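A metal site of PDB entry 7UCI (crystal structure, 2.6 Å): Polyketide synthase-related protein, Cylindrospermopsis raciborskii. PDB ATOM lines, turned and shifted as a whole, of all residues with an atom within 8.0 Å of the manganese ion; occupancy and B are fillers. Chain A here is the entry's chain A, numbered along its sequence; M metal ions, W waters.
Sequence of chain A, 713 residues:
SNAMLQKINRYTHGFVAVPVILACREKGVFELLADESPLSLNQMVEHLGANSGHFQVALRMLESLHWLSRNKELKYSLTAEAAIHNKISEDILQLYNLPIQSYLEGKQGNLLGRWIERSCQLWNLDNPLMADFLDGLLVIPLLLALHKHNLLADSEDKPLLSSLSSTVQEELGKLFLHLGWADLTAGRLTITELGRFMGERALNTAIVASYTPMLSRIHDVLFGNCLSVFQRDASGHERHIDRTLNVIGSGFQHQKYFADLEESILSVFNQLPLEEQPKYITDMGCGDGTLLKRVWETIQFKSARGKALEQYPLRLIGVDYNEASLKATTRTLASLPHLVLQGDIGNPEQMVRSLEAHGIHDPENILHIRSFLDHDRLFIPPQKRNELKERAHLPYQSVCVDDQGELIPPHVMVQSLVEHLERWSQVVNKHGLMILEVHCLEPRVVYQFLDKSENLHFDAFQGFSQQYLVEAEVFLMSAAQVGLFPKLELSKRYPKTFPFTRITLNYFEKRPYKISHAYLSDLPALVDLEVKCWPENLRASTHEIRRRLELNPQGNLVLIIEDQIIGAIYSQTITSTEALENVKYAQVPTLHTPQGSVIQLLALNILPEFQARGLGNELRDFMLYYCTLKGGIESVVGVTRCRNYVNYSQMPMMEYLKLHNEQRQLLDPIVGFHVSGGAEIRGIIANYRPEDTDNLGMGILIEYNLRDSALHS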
ATOM      1  N   TYR A 211      19.528 -16.826 -26.347  1.00  0.00           N
ATOM      2  CA  TYR A 211      18.162 -16.994 -25.865  1.00  0.00           C
ATOM      3  C   TYR A 211      17.277 -15.830 -26.258  1.00  0.00           C
ATOM      4  O   TYR A 211      16.055 -15.897 -26.046  1.00  0.00           O
ATOM      5  CB  TYR A 211      18.147 -17.168 -24.345  1.00  0.00           C
ATOM      6  CG  TYR A 211      18.996 -18.325 -23.839  1.00  0.00           C
ATOM      7  CD1 TYR A 211      19.488 -19.289 -24.704  1.00  0.00           C
ATOM      8  CD2 TYR A 211      19.295 -18.459 -22.487  1.00  0.00           C
ATOM      9  CE1 TYR A 211      20.257 -20.340 -24.254  1.00  0.00           C
ATOM     10  CE2 TYR A 211      20.067 -19.509 -22.022  1.00  0.00           C
ATOM     11  CZ  TYR A 211      20.536 -20.451 -22.907  1.00  0.00           C
ATOM     12  OH  TYR A 211      21.308 -21.501 -22.443  1.00  0.00           O
ATOM     13  N   SER A 371      28.450 -35.780 -25.076  1.00  0.00           N
ATOM     14  CA  SER A 371      28.626 -34.576 -24.245  1.00  0.00           C
ATOM     15  C   SER A 371      27.359 -33.731 -24.254  1.00  0.00           C
ATOM     16  O   SER A 371      27.121 -32.947 -25.180  1.00  0.00           O
ATOM     17  CB  SER A 371      29.825 -33.777 -24.730  1.00  0.00           C
ATOM     18  OG  SER A 371      30.017 -32.610 -23.948  1.00  0.00           O
ATOM     19  N   PHE A 372      26.556 -33.879 -23.194  1.00  0.00           N
ATOM     20  CA  PHE A 372      25.453 -32.959 -22.883  1.00  0.00           C
ATOM     21  C   PHE A 372      24.340 -33.046 -23.922  1.00  0.00           C
ATOM     22  O   PHE A 372      23.889 -32.027 -24.463  1.00  0.00           O
ATOM     23  CB  PHE A 372      25.959 -31.523 -22.750  1.00  0.00           C
ATOM     24  CG  PHE A 372      26.923 -31.308 -21.620  1.00  0.00           C
ATOM     25  CD1 PHE A 372      26.475 -31.276 -20.309  1.00  0.00           C
ATOM     26  CD2 PHE A 372      28.274 -31.144 -21.869  1.00  0.00           C
ATOM     27  CE1 PHE A 372      27.365 -31.077 -19.267  1.00  0.00           C
ATOM     28  CE2 PHE A 372      29.168 -30.954 -20.827  1.00  0.00           C
ATOM     29  CZ  PHE A 372      28.709 -30.917 -19.522  1.00  0.00           C
ATOM     30  N   LEU A 373      23.875 -34.262 -24.197  1.00  0.00           N
ATOM     31  CA  LEU A 373      22.844 -34.453 -25.203  1.00  0.00           C
ATOM     32  C   LEU A 373      21.681 -35.347 -24.773  1.00  0.00           C
ATOM     33  O   LEU A 373      20.597 -35.223 -25.354  1.00  0.00           O
ATOM     34  CB  LEU A 373      23.452 -35.041 -26.481  1.00  0.00           C
ATOM     35  CG  LEU A 373      22.629 -34.943 -27.769  1.00  0.00           C
ATOM     36  CD1 LEU A 373      22.327 -33.502 -28.128  1.00  0.00           C
ATOM     37  CD2 LEU A 373      23.401 -35.637 -28.890  1.00  0.00           C
ATOM     38  N   ASP A 374      21.864 -36.224 -23.786  1.00  0.00           N
ATOM     39  CA  ASP A 374      20.761 -37.077 -23.355  1.00  0.00           C
ATOM     40  C   ASP A 374      19.527 -36.277 -22.991  1.00  0.00           C
ATOM     41  O   ASP A 374      18.394 -36.751 -23.171  1.00  0.00           O
ATOM     42  CB  ASP A 374      21.181 -37.923 -22.149  1.00  0.00           C
ATOM     43  CG  ASP A 374      22.089 -39.063 -22.539  1.00  0.00           C
ATOM     44  OD1 ASP A 374      21.582 -40.081 -23.048  1.00  0.00           O
ATOM     45  OD2 ASP A 374      23.308 -38.925 -22.355  1.00  0.00           O
ATOM     46  N   HIS A 375      19.708 -35.063 -22.470  1.00  0.00           N
ATOM     47  CA  HIS A 375      18.587 -34.196 -22.137  1.00  0.00           C
ATOM     48  C   HIS A 375      17.987 -33.530 -23.362  1.00  0.00           C
ATOM     49  O   HIS A 375      16.904 -32.949 -23.260  1.00  0.00           O
ATOM     50  CB  HIS A 375      19.029 -33.137 -21.132  1.00  0.00           C
ATOM     51  CG  HIS A 375      20.024 -32.161 -21.681  1.00  0.00           C
ATOM     52  ND1 HIS A 375      21.378 -32.440 -21.767  1.00  0.00           N
ATOM     53  CD2 HIS A 375      19.874 -30.903 -22.169  1.00  0.00           C
ATOM     54  CE1 HIS A 375      22.003 -31.401 -22.284  1.00  0.00           C
ATOM     55  NE2 HIS A 375      21.119 -30.458 -22.534  1.00  0.00           N
ATOM     56  N   ASP A 376      18.665 -33.590 -24.512  1.00  0.00           N
ATOM     57  CA  ASP A 376      18.146 -33.050 -25.760  1.00  0.00           C
ATOM     58  C   ASP A 376      17.660 -34.142 -26.704  1.00  0.00           C
ATOM     59  O   ASP A 376      17.388 -33.859 -27.873  1.00  0.00           O
ATOM     60  CB  ASP A 376      19.213 -32.197 -26.445  1.00  0.00           C
ATOM     61  CG  ASP A 376      18.618 -31.098 -27.308  1.00  0.00           C
ATOM     62  OD1 ASP A 376      17.455 -31.245 -27.751  1.00  0.00           O
ATOM     63  OD2 ASP A 376      19.313 -30.087 -27.546  1.00  0.00           O
ATOM     64  N   GLU A 437      26.958 -34.952 -18.637  1.00  0.00           N
ATOM     65  CA  GLU A 437      25.562 -34.540 -18.672  1.00  0.00           C
ATOM     66  C   GLU A 437      25.311 -33.455 -17.633  1.00  0.00           C
ATOM     67  O   GLU A 437      26.034 -33.361 -16.641  1.00  0.00           O
ATOM     68  CB  GLU A 437      24.619 -35.718 -18.444  1.00  0.00           C
ATOM     69  CG  GLU A 437      23.139 -35.371 -18.538  1.00  0.00           C
ATOM     70  CD  GLU A 437      22.794 -34.667 -19.835  1.00  0.00           C
ATOM     71  OE1 GLU A 437      23.485 -34.909 -20.849  1.00  0.00           O
ATOM     72  OE2 GLU A 437      21.831 -33.873 -19.851  1.00  0.00           O
ATOM     73  N   VAL A 438      24.293 -32.635 -17.894  1.00  0.00           N
ATOM     74  CA  VAL A 438      23.919 -31.535 -17.024  1.00  0.00           C
ATOM     75  C   VAL A 438      22.581 -31.854 -16.375  1.00  0.00           C
ATOM     76  O   VAL A 438      21.775 -32.630 -16.902  1.00  0.00           O
ATOM     77  CB  VAL A 438      23.852 -30.207 -17.804  1.00  0.00           C
ATOM     78  CG1 VAL A 438      22.843 -30.300 -18.938  1.00  0.00           C
ATOM     79  CG2 VAL A 438      23.526 -29.049 -16.875  1.00  0.00           C
ATOM     80  N   PHE A 458      19.792 -21.309 -16.681  1.00  0.00           N
ATOM     81  CA  PHE A 458      19.998 -22.470 -17.540  1.00  0.00           C
ATOM     82  C   PHE A 458      18.846 -23.463 -17.412  1.00  0.00           C
ATOM     83  O   PHE A 458      18.312 -23.932 -18.420  1.00  0.00           O
ATOM     84  CB  PHE A 458      21.329 -23.145 -17.198  1.00  0.00           C
ATOM     85  CG  PHE A 458      21.746 -24.202 -18.187  1.00  0.00           C
ATOM     86  CD1 PHE A 458      22.452 -23.858 -19.321  1.00  0.00           C
ATOM     87  CD2 PHE A 458      21.413 -25.525 -17.983  1.00  0.00           C
ATOM     88  CE1 PHE A 458      22.836 -24.819 -20.241  1.00  0.00           C
ATOM     89  CE2 PHE A 458      21.796 -26.498 -18.895  1.00  0.00           C
ATOM     90  CZ  PHE A 458      22.498 -26.145 -20.030  1.00  0.00           C
ATOM     91  N   PHE A 461      15.751 -21.941 -19.144  1.00  0.00           N
ATOM     92  CA  PHE A 461      15.707 -21.962 -20.601  1.00  0.00           C
ATOM     93  C   PHE A 461      15.578 -23.384 -21.139  1.00  0.00           C
ATOM     94  O   PHE A 461      14.747 -23.653 -22.019  1.00  0.00           O
ATOM     95  CB  PHE A 461      16.938 -21.293 -21.201  1.00  0.00           C
ATOM     96  CG  PHE A 461      16.871 -21.136 -22.693  1.00  0.00           C
ATOM     97  CD1 PHE A 461      16.150 -20.096 -23.251  1.00  0.00           C
ATOM     98  CD2 PHE A 461      17.494 -22.046 -23.533  1.00  0.00           C
ATOM     99  CE1 PHE A 461      16.070 -19.943 -24.618  1.00  0.00           C
ATOM    100  CE2 PHE A 461      17.412 -21.894 -24.914  1.00  0.00           C
ATOM    101  CZ  PHE A 461      16.695 -20.840 -25.452  1.00  0.00           C
ATOM    102  N   GLN A 462      16.408 -24.305 -20.624  1.00  0.00           N
ATOM    103  CA  GLN A 462      16.389 -25.672 -21.113  1.00  0.00           C
ATOM    104  C   GLN A 462      15.021 -26.324 -20.910  1.00  0.00           C
ATOM    105  O   GLN A 462      14.673 -27.267 -21.638  1.00  0.00           O
ATOM    106  CB  GLN A 462      17.494 -26.465 -20.437  1.00  0.00           C
ATOM    107  CG  GLN A 462      18.887 -25.833 -20.606  1.00  0.00           C
ATOM    108  CD  GLN A 462      19.645 -26.346 -21.828  1.00  0.00           C
ATOM    109  OE1 GLN A 462      19.995 -27.524 -21.896  1.00  0.00           O
ATOM    110  NE2 GLN A 462      19.899 -25.464 -22.783  1.00  0.00           N
ATOM    111  N   SER A 465      12.918 -24.571 -23.631  1.00  0.00           N
ATOM    112  CA  SER A 465      13.329 -25.068 -24.943  1.00  0.00           C
ATOM    113  C   SER A 465      13.004 -26.538 -25.145  1.00  0.00           C
ATOM    114  O   SER A 465      13.492 -27.147 -26.114  1.00  0.00           O
ATOM    115  CB  SER A 465      14.828 -24.841 -25.142  1.00  0.00           C
ATOM    116  OG  SER A 465      15.580 -25.934 -24.642  1.00  0.00           O
ATOM    117  N   GLN A 467      13.970 -29.173 -23.615  1.00  0.00           N
ATOM    118  CA  GLN A 467      15.021 -30.120 -23.226  1.00  0.00           C
ATOM    119  C   GLN A 467      14.711 -30.644 -21.835  1.00  0.00           C
ATOM    120  O   GLN A 467      13.962 -30.044 -21.068  1.00  0.00           O
ATOM    121  CB  GLN A 467      16.395 -29.450 -23.273  1.00  0.00           C
ATOM    122  CG  GLN A 467      16.771 -28.984 -24.676  1.00  0.00           C
ATOM    123  CD  GLN A 467      18.228 -28.632 -24.815  1.00  0.00           C
ATOM    124  OE1 GLN A 467      18.997 -28.728 -23.863  1.00  0.00           O
ATOM    125  NE2 GLN A 467      18.630 -28.215 -26.009  1.00  0.00           N
ATOM    126  N   TYR A 468      15.284 -31.806 -21.516  1.00  0.00           N
ATOM    127  CA  TYR A 468      14.804 -32.619 -20.402  1.00  0.00           C
ATOM    128  C   TYR A 468      15.911 -32.837 -19.384  1.00  0.00           C
ATOM    129  O   TYR A 468      16.739 -33.746 -19.524  1.00  0.00           O
ATOM    130  CB  TYR A 468      14.267 -33.943 -20.936  1.00  0.00           C
ATOM    131  CG  TYR A 468      13.326 -33.734 -22.108  1.00  0.00           C
ATOM    132  CD1 TYR A 468      12.254 -32.869 -22.013  1.00  0.00           C
ATOM    133  CD2 TYR A 468      13.530 -34.398 -23.308  1.00  0.00           C
ATOM    134  CE1 TYR A 468      11.397 -32.672 -23.075  1.00  0.00           C
ATOM    135  CE2 TYR A 468      12.676 -34.212 -24.384  1.00  0.00           C
ATOM    136  CZ  TYR A 468      11.608 -33.344 -24.261  1.00  0.00           C
ATOM    137  OH  TYR A 468      10.759 -33.144 -25.318  1.00  0.00           O
ATOM    138  N   LEU A 469      15.899 -32.024 -18.336  1.00  0.00           N
ATOM    139  CA  LEU A 469      16.896 -32.084 -17.280  1.00  0.00           C
ATOM    140  C   LEU A 469      16.346 -32.830 -16.068  1.00  0.00           C
ATOM    141  O   LEU A 469      15.217 -32.568 -15.627  1.00  0.00           O
ATOM    142  CB  LEU A 469      17.330 -30.680 -16.859  1.00  0.00           C
ATOM    143  CG  LEU A 469      18.263 -29.896 -17.783  1.00  0.00           C
ATOM    144  CD1 LEU A 469      18.690 -28.613 -17.062  1.00  0.00           C
ATOM    145  CD2 LEU A 469      19.465 -30.724 -18.175  1.00  0.00           C
HETATM  146 MN    MN M   1      20.937 -28.338 -24.053  1.00  0.00          MN
HETATM  147  O   HOH W   1      21.519 -29.688 -25.414  1.00  0.00           O
HETATM  148  O   HOH W   2      21.973 -26.804 -25.967  1.00  0.00           O
HETATM  149  O   HOH W   3      23.142 -28.074 -22.691  1.00  0.00           O
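Within 4 Å of the manganese ion: His 375, Gln 462 and Gln 467.
The nearest printed residue that does not touch the manganese ion is Asp 376 (4.2 Å).
OG of Ser 465 is in hydrogen-bond range of O of Gln 462 (3.4 Å).
OD2 of Asp 376 lies within hydrogen-bond range of NE2 of Gln 467, at 2.5 Å.
A ring nitrogen (ND1) of His 375 lies within hydrogen-bond range of the side-chain carboxylate (OE2) of Glu 437.
O of His 375 is in hydrogen-bond range of N of Tyr 468, at 2.6 Å.
Water W1 lies within hydrogen-bond range of OD2 of Asp 376, NE2 of Gln 467 and O of Phe 372.
The manganese ion is bound by the side-chain amide oxygen (OE1) of Gln 467 (2.0 Å), water W1 (2.0 Å), the side-chain amide oxygen (OE1) of Gln 462 (2.5 Å), water W3 (2.6 Å), a ring nitrogen (NE2) of His 375 (2.6 Å) and water W2 (2.7 Å).
The manganese ion has six donor atoms within binding distance.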
